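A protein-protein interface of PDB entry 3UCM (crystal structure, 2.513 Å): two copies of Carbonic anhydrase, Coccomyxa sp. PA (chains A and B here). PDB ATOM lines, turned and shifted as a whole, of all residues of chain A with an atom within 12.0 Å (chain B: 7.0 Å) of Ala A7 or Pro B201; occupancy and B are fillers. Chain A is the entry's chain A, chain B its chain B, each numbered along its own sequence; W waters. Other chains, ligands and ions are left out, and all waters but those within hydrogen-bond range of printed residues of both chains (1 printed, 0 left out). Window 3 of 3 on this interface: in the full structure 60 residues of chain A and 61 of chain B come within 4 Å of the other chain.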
ATOM      1  N   THR A   6     -19.884  21.951  10.344  1.00  0.00           N
ATOM      2  CA  THR A   6     -19.987  20.574  10.954  1.00  0.00           C
ATOM      3  C   THR A   6     -18.994  19.519  10.371  1.00  0.00           C
ATOM      4  O   THR A   6     -18.950  18.374  10.844  1.00  0.00           O
ATOM      5  CB  THR A   6     -21.509  20.051  11.044  1.00  0.00           C
ATOM      6  OG1 THR A   6     -21.564  18.683  11.519  1.00  0.00           O
ATOM      7  CG2 THR A   6     -22.316  20.224   9.686  1.00  0.00           C
ATOM      8  N   ALA A   7     -18.210  19.921   9.363  1.00  0.00           N
ATOM      9  CA  ALA A   7     -17.065  19.142   8.865  1.00  0.00           C
ATOM     10  C   ALA A   7     -15.822  19.306   9.750  1.00  0.00           C
ATOM     11  O   ALA A   7     -14.700  18.956   9.357  1.00  0.00           O
ATOM     12  CB  ALA A   7     -16.740  19.567   7.457  1.00  0.00           C
ATOM     13  N   ASP A   8     -16.035  19.826  10.953  1.00  0.00           N
ATOM     14  CA  ASP A   8     -14.963  20.278  11.848  1.00  0.00           C
ATOM     15  C   ASP A   8     -14.415  19.143  12.770  1.00  0.00           C
ATOM     16  O   ASP A   8     -15.185  18.310  13.261  1.00  0.00           O
ATOM     17  CB  ASP A   8     -15.500  21.493  12.632  1.00  0.00           C
ATOM     18  CG  ASP A   8     -14.565  21.977  13.700  1.00  0.00           C
ATOM     19  OD1 ASP A   8     -13.360  22.160  13.435  1.00  0.00           O
ATOM     20  OD2 ASP A   8     -15.049  22.187  14.812  1.00  0.00           O
ATOM     21  N   LEU A   9     -13.094  19.126  12.976  1.00  0.00           N
ATOM     22  CA  LEU A   9     -12.393  18.023  13.673  1.00  0.00           C
ATOM     23  C   LEU A   9     -12.074  18.220  15.166  1.00  0.00           C
ATOM     24  O   LEU A   9     -11.592  17.291  15.841  1.00  0.00           O
ATOM     25  CB  LEU A   9     -11.088  17.697  12.954  1.00  0.00           C
ATOM     26  CG  LEU A   9     -11.183  17.011  11.596  1.00  0.00           C
ATOM     27  CD1 LEU A   9      -9.790  16.858  11.050  1.00  0.00           C
ATOM     28  CD2 LEU A   9     -11.894  15.681  11.696  1.00  0.00           C
ATOM     29  N   SER A  10     -12.361  19.423  15.663  1.00  0.00           N
ATOM     30  CA  SER A  10     -12.129  19.803  17.057  1.00  0.00           C
ATOM     31  C   SER A  10     -12.637  18.755  18.051  1.00  0.00           C
ATOM     32  O   SER A  10     -11.925  18.417  18.995  1.00  0.00           O
ATOM     33  CB  SER A  10     -12.777  21.149  17.355  1.00  0.00           C
ATOM     34  OG  SER A  10     -12.108  22.166  16.656  1.00  0.00           O
ATOM     35  N   PRO A  11     -13.872  18.244  17.860  1.00  0.00           N
ATOM     36  CA  PRO A  11     -14.257  17.294  18.887  1.00  0.00           C
ATOM     37  C   PRO A  11     -13.355  16.088  18.807  1.00  0.00           C
ATOM     38  O   PRO A  11     -13.037  15.498  19.839  1.00  0.00           O
ATOM     39  CB  PRO A  11     -15.702  16.923  18.518  1.00  0.00           C
ATOM     40  CG  PRO A  11     -16.181  18.093  17.705  1.00  0.00           C
ATOM     41  CD  PRO A  11     -14.971  18.519  16.914  1.00  0.00           C
ATOM     42  N   LEU A  12     -12.910  15.748  17.602  1.00  0.00           N
ATOM     43  CA  LEU A  12     -12.245  14.460  17.420  1.00  0.00           C
ATOM     44  C   LEU A  12     -10.809  14.563  17.924  1.00  0.00           C
ATOM     45  O   LEU A  12     -10.308  13.600  18.505  1.00  0.00           O
ATOM     46  CB  LEU A  12     -12.276  13.997  15.957  1.00  0.00           C
ATOM     47  CG  LEU A  12     -12.633  12.566  15.563  1.00  0.00           C
ATOM     48  CD1 LEU A  12     -11.861  12.250  14.318  1.00  0.00           C
ATOM     49  CD2 LEU A  12     -12.274  11.581  16.633  1.00  0.00           C
ATOM     50  N   LEU A  13     -10.177  15.726  17.709  1.00  0.00           N
ATOM     51  CA  LEU A  13      -8.855  16.013  18.241  1.00  0.00           C
ATOM     52  C   LEU A  13      -8.822  16.111  19.781  1.00  0.00           C
ATOM     53  O   LEU A  13      -7.782  15.806  20.415  1.00  0.00           O
ATOM     54  CB  LEU A  13      -8.301  17.274  17.644  1.00  0.00           C
ATOM     55  CG  LEU A  13      -8.129  17.345  16.119  1.00  0.00           C
ATOM     56  CD1 LEU A  13      -7.635  18.739  15.683  1.00  0.00           C
ATOM     57  CD2 LEU A  13      -7.208  16.260  15.568  1.00  0.00           C
ATOM     58  N   TYR B  42     -17.156   7.938   9.552  1.00  0.00           N
ATOM     59  CA  TYR B  42     -15.754   8.121   9.162  1.00  0.00           C
ATOM     60  C   TYR B  42     -15.183   6.938   8.362  1.00  0.00           C
ATOM     61  O   TYR B  42     -15.493   5.763   8.633  1.00  0.00           O
ATOM     62  CB  TYR B  42     -14.899   8.300  10.430  1.00  0.00           C
ATOM     63  CG  TYR B  42     -15.170   9.597  11.141  1.00  0.00           C
ATOM     64  CD1 TYR B  42     -16.098   9.662  12.190  1.00  0.00           C
ATOM     65  CD2 TYR B  42     -14.543  10.772  10.727  1.00  0.00           C
ATOM     66  CE1 TYR B  42     -16.376  10.867  12.830  1.00  0.00           C
ATOM     67  CE2 TYR B  42     -14.813  11.981  11.344  1.00  0.00           C
ATOM     68  CZ  TYR B  42     -15.734  12.016  12.404  1.00  0.00           C
ATOM     69  OH  TYR B  42     -16.010  13.216  13.002  1.00  0.00           O
ATOM     70  N   LYS B  96     -19.433  10.401   5.633  1.00  0.00           N
ATOM     71  CA  LYS B  96     -19.397  11.862   5.483  1.00  0.00           C
ATOM     72  C   LYS B  96     -17.992  12.445   5.525  1.00  0.00           C
ATOM     73  O   LYS B  96     -17.762  13.545   4.953  1.00  0.00           O
ATOM     74  CB  LYS B  96     -20.217  12.519   6.587  1.00  0.00           C
ATOM     75  CG  LYS B  96     -21.730  12.328   6.528  1.00  0.00           C
ATOM     76  CD  LYS B  96     -22.353  12.662   7.902  1.00  0.00           C
ATOM     77  CE  LYS B  96     -23.879  12.356   7.966  1.00  0.00           C
ATOM     78  NZ  LYS B  96     -24.265  12.049   9.378  1.00  0.00           N
ATOM     79  N   HIS B  97     -17.058  11.747   6.207  1.00  0.00           N
ATOM     80  CA  HIS B  97     -15.679  12.265   6.388  1.00  0.00           C
ATOM     81  C   HIS B  97     -14.609  11.212   6.135  1.00  0.00           C
ATOM     82  O   HIS B  97     -14.649  10.101   6.717  1.00  0.00           O
ATOM     83  CB  HIS B  97     -15.470  12.828   7.792  1.00  0.00           C
ATOM     84  CG  HIS B  97     -16.614  13.652   8.307  1.00  0.00           C
ATOM     85  ND1 HIS B  97     -17.388  13.264   9.384  1.00  0.00           N
ATOM     86  CD2 HIS B  97     -17.107  14.846   7.905  1.00  0.00           C
ATOM     87  CE1 HIS B  97     -18.318  14.179   9.613  1.00  0.00           C
ATOM     88  NE2 HIS B  97     -18.172  15.143   8.724  1.00  0.00           N
ATOM     89  N   SER B 182     -16.371  15.210   3.048  1.00  0.00           N
ATOM     90  CA  SER B 182     -15.158  16.028   3.347  1.00  0.00           C
ATOM     91  C   SER B 182     -13.858  15.205   3.403  1.00  0.00           C
ATOM     92  O   SER B 182     -13.896  14.031   3.724  1.00  0.00           O
ATOM     93  CB  SER B 182     -15.320  16.689   4.713  1.00  0.00           C
ATOM     94  OG  SER B 182     -15.400  15.692   5.741  1.00  0.00           O
ATOM     95  N   VAL B 183     -12.716  15.831   3.134  1.00  0.00           N
ATOM     96  CA  VAL B 183     -11.428  15.130   3.141  1.00  0.00           C
ATOM     97  C   VAL B 183     -10.407  15.928   3.989  1.00  0.00           C
ATOM     98  O   VAL B 183     -10.274  17.117   3.789  1.00  0.00           O
ATOM     99  CB  VAL B 183     -10.874  14.879   1.691  1.00  0.00           C
ATOM    100  CG1 VAL B 183      -9.729  13.864   1.712  1.00  0.00           C
ATOM    101  CG2 VAL B 183     -11.993  14.476   0.649  1.00  0.00           C
ATOM    102  N   HIS B 184      -9.654  15.247   4.866  1.00  0.00           N
ATOM    103  CA  HIS B 184      -8.820  15.844   5.934  1.00  0.00           C
ATOM    104  C   HIS B 184      -7.403  15.195   6.024  1.00  0.00           C
ATOM    105  O   HIS B 184      -7.292  13.989   6.325  1.00  0.00           O
ATOM    106  CB  HIS B 184      -9.477  15.573   7.310  1.00  0.00           C
ATOM    107  CG  HIS B 184     -10.950  15.830   7.356  1.00  0.00           C
ATOM    108  ND1 HIS B 184     -11.482  17.068   7.653  1.00  0.00           N
ATOM    109  CD2 HIS B 184     -12.003  15.002   7.165  1.00  0.00           C
ATOM    110  CE1 HIS B 184     -12.798  16.993   7.626  1.00  0.00           C
ATOM    111  NE2 HIS B 184     -13.140  15.746   7.352  1.00  0.00           N
ATOM    112  N   GLY B 185      -6.355  15.997   5.823  1.00  0.00           N
ATOM    113  CA  GLY B 185      -4.981  15.562   6.001  1.00  0.00           C
ATOM    114  C   GLY B 185      -4.458  15.710   7.426  1.00  0.00           C
ATOM    115  O   GLY B 185      -4.364  16.828   7.952  1.00  0.00           O
ATOM    116  N   GLU B 197      -3.263  18.304  12.780  1.00  0.00           N
ATOM    117  CA  GLU B 197      -3.980  18.534  11.492  1.00  0.00           C
ATOM    118  C   GLU B 197      -3.180  19.347  10.433  1.00  0.00           C
ATOM    119  O   GLU B 197      -3.005  20.546  10.611  1.00  0.00           O
ATOM    120  CB  GLU B 197      -5.319  19.230  11.790  1.00  0.00           C
ATOM    121  CG  GLU B 197      -6.195  19.583  10.566  1.00  0.00           C
ATOM    122  CD  GLU B 197      -7.252  20.642  10.882  1.00  0.00           C
ATOM    123  OE1 GLU B 197      -6.853  21.803  11.135  1.00  0.00           O
ATOM    124  OE2 GLU B 197      -8.476  20.342  10.874  1.00  0.00           O
ATOM    125  N   ILE B 199      -3.751  19.884   6.938  1.00  0.00           N
ATOM    126  CA  ILE B 199      -4.570  20.494   5.903  1.00  0.00           C
ATOM    127  C   ILE B 199      -6.024  20.566   6.402  1.00  0.00           C
ATOM    128  O   ILE B 199      -6.630  19.567   6.845  1.00  0.00           O
ATOM    129  CB  ILE B 199      -4.554  19.691   4.598  1.00  0.00           C
ATOM    130  CG1 ILE B 199      -3.132  19.419   4.130  1.00  0.00           C
ATOM    131  CG2 ILE B 199      -5.301  20.460   3.487  1.00  0.00           C
ATOM    132  CD1 ILE B 199      -3.047  18.441   2.956  1.00  0.00           C
ATOM    133  N   LYS B 200      -6.579  21.767   6.349  1.00  0.00           N
ATOM    134  CA  LYS B 200      -7.928  22.013   6.826  1.00  0.00           C
ATOM    135  C   LYS B 200      -8.938  21.263   5.968  1.00  0.00           C
ATOM    136  O   LYS B 200      -8.597  20.821   4.866  1.00  0.00           O
ATOM    137  CB  LYS B 200      -8.205  23.526   6.830  1.00  0.00           C
ATOM    138  CG  LYS B 200      -7.231  24.288   7.743  1.00  0.00           C
ATOM    139  CD  LYS B 200      -7.918  25.511   8.419  1.00  0.00           C
ATOM    140  CE  LYS B 200      -6.892  26.483   9.137  1.00  0.00           C
ATOM    141  NZ  LYS B 200      -7.580  27.715   9.669  1.00  0.00           N
ATOM    142  N   PRO B 201     -10.177  21.095   6.473  1.00  0.00           N
ATOM    143  CA  PRO B 201     -11.231  20.344   5.704  1.00  0.00           C
ATOM    144  C   PRO B 201     -11.440  20.774   4.231  1.00  0.00           C
ATOM    145  O   PRO B 201     -11.397  21.970   3.898  1.00  0.00           O
ATOM    146  CB  PRO B 201     -12.513  20.582   6.524  1.00  0.00           C
ATOM    147  CG  PRO B 201     -12.006  20.780   7.973  1.00  0.00           C
ATOM    148  CD  PRO B 201     -10.630  21.482   7.825  1.00  0.00           C
ATOM    149  N   ILE B 202     -11.633  19.794   3.350  1.00  0.00           N
ATOM    150  CA  ILE B 202     -11.868  20.054   1.928  1.00  0.00           C
ATOM    151  C   ILE B 202     -13.226  19.445   1.665  1.00  0.00           C
ATOM    152  O   ILE B 202     -13.406  18.268   1.923  1.00  0.00           O
ATOM    153  CB  ILE B 202     -10.735  19.459   1.010  1.00  0.00           C
ATOM    154  CG1 ILE B 202      -9.383  20.139   1.327  1.00  0.00           C
ATOM    155  CG2 ILE B 202     -11.115  19.617  -0.444  1.00  0.00           C
ATOM    156  CD1 ILE B 202      -8.200  19.833   0.412  1.00  0.00           C
ATOM    157  N   THR B 203     -14.188  20.259   1.223  1.00  0.00           N
ATOM    158  CA  THR B 203     -15.587  19.831   1.048  1.00  0.00           C
ATOM    159  C   THR B 203     -16.102  19.852  -0.409  1.00  0.00           C
ATOM    160  O   THR B 203     -17.248  19.446  -0.693  1.00  0.00           O
ATOM    161  CB  THR B 203     -16.529  20.688   1.913  1.00  0.00           C
ATOM    162  OG1 THR B 203     -16.645  22.020   1.355  1.00  0.00           O
ATOM    163  CG2 THR B 203     -16.007  20.746   3.360  1.00  0.00           C
ATOM    164  N   GLY B 204     -15.258  20.333  -1.313  1.00  0.00           N
ATOM    165  CA  GLY B 204     -15.565  20.328  -2.725  1.00  0.00           C
ATOM    166  C   GLY B 204     -14.407  20.902  -3.494  1.00  0.00           C
ATOM    167  O   GLY B 204     -13.316  21.121  -2.938  1.00  0.00           O
ATOM    168  N   ASP B 207     -12.695  24.619  -1.963  1.00  0.00           N
ATOM    169  CA  ASP B 207     -11.707  24.336  -0.904  1.00  0.00           C
ATOM    170  C   ASP B 207     -10.429  23.705  -1.497  1.00  0.00           C
ATOM    171  O   ASP B 207      -9.295  24.076  -1.146  1.00  0.00           O
ATOM    172  CB  ASP B 207     -12.263  23.367   0.144  1.00  0.00           C
ATOM    173  CG  ASP B 207     -13.448  23.925   0.942  1.00  0.00           C
ATOM    174  OD1 ASP B 207     -13.529  25.130   1.238  1.00  0.00           O
ATOM    175  OD2 ASP B 207     -14.301  23.122   1.337  1.00  0.00           O
ATOM    176  N   ALA B 208     -10.588  22.747  -2.409  1.00  0.00           N
ATOM    177  CA  ALA B 208      -9.402  22.119  -2.987  1.00  0.00           C
ATOM    178  C   ALA B 208      -8.483  23.131  -3.754  1.00  0.00           C
ATOM    179  O   ALA B 208      -7.263  23.059  -3.648  1.00  0.00           O
ATOM    180  CB  ALA B 208      -9.798  20.898  -3.830  1.00  0.00           C
ATOM    181  N   LEU B 211      -6.637  25.103  -0.797  1.00  0.00           N
ATOM    182  CA  LEU B 211      -5.827  24.358   0.176  1.00  0.00           C
ATOM    183  C   LEU B 211      -4.651  23.487  -0.339  1.00  0.00           C
ATOM    184  O   LEU B 211      -3.668  23.298   0.412  1.00  0.00           O
ATOM    185  CB  LEU B 211      -6.734  23.587   1.146  1.00  0.00           C
ATOM    186  CG  LEU B 211      -7.565  24.542   2.042  1.00  0.00           C
ATOM    187  CD1 LEU B 211      -8.742  23.870   2.677  1.00  0.00           C
ATOM    188  CD2 LEU B 211      -6.705  25.295   3.134  1.00  0.00           C
HETATM  189  O   HOH W   1     -11.145  21.307  11.388  1.00  0.00           O
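NE2 of His B184 lies within hydrogen-bond range of OG of Ser B182 (2.8 Å).
Among the printed residues, pairs that only touch across the chains: Thr A6 with His B97 (3.9 Å), Ala A7 with His B184 (3.2 Å), Ala A7 with Pro B201 (3.5 Å), Leu A9 with His B184 (3.8 Å) and Leu A9 with Glu B197 (3.7 Å).
Ala A7 touches just these residues of chain B: His B184 (3.2 Å) and Pro B201 (3.5 Å).
Of chain A, only Ala A7 comes within 4 Å of Pro B201.
No residue of chain A comes within 4 Å of Ser B182.
No residue of chain A comes within 4 Å of Val B183.
No residue of chain A comes within 4 Å of Lys B200.
No residue of chain A comes within 4 Å of Ile B202.
No residue of chain A comes within 4 Å of Thr B203.
No residue of chain A comes within 4 Å of Asp B207.
Of the printed residues of chain B, Thr A6 touches His B97 (3.9 Å).
Of the printed residues of chain A, Glu B197 touches Leu A9 (3.7 Å).
Printed residues of chain A within 4 Å of His B97: Thr A6.
Of the printed residues of chain B, Leu A9 touches His B184 and Glu B197.
Leu A13 touches none of the printed residues of chain B.
Pro A11 touches none of the printed residues of chain B.
The nearest residue of chain B that does not touch Ala A7 is His B97 (4.2 Å).
Hydrophobic or aromatic side chains of chain A that line the printed part of chain B: Leu A9.
Of the 17 printed residues of chain B, 4 touch a printed residue of chain A.
Among the printed residues, 5 pairs touch across the chains.
No position is printed for both chains.
Water W1 lies within hydrogen-bond range of the side-chain carboxylate of Glu B197 (2.9 Å), the side-chain carboxylate of Asp A8 (3.1 Å) and the backbone NH of Leu A9 (3.3 Å).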
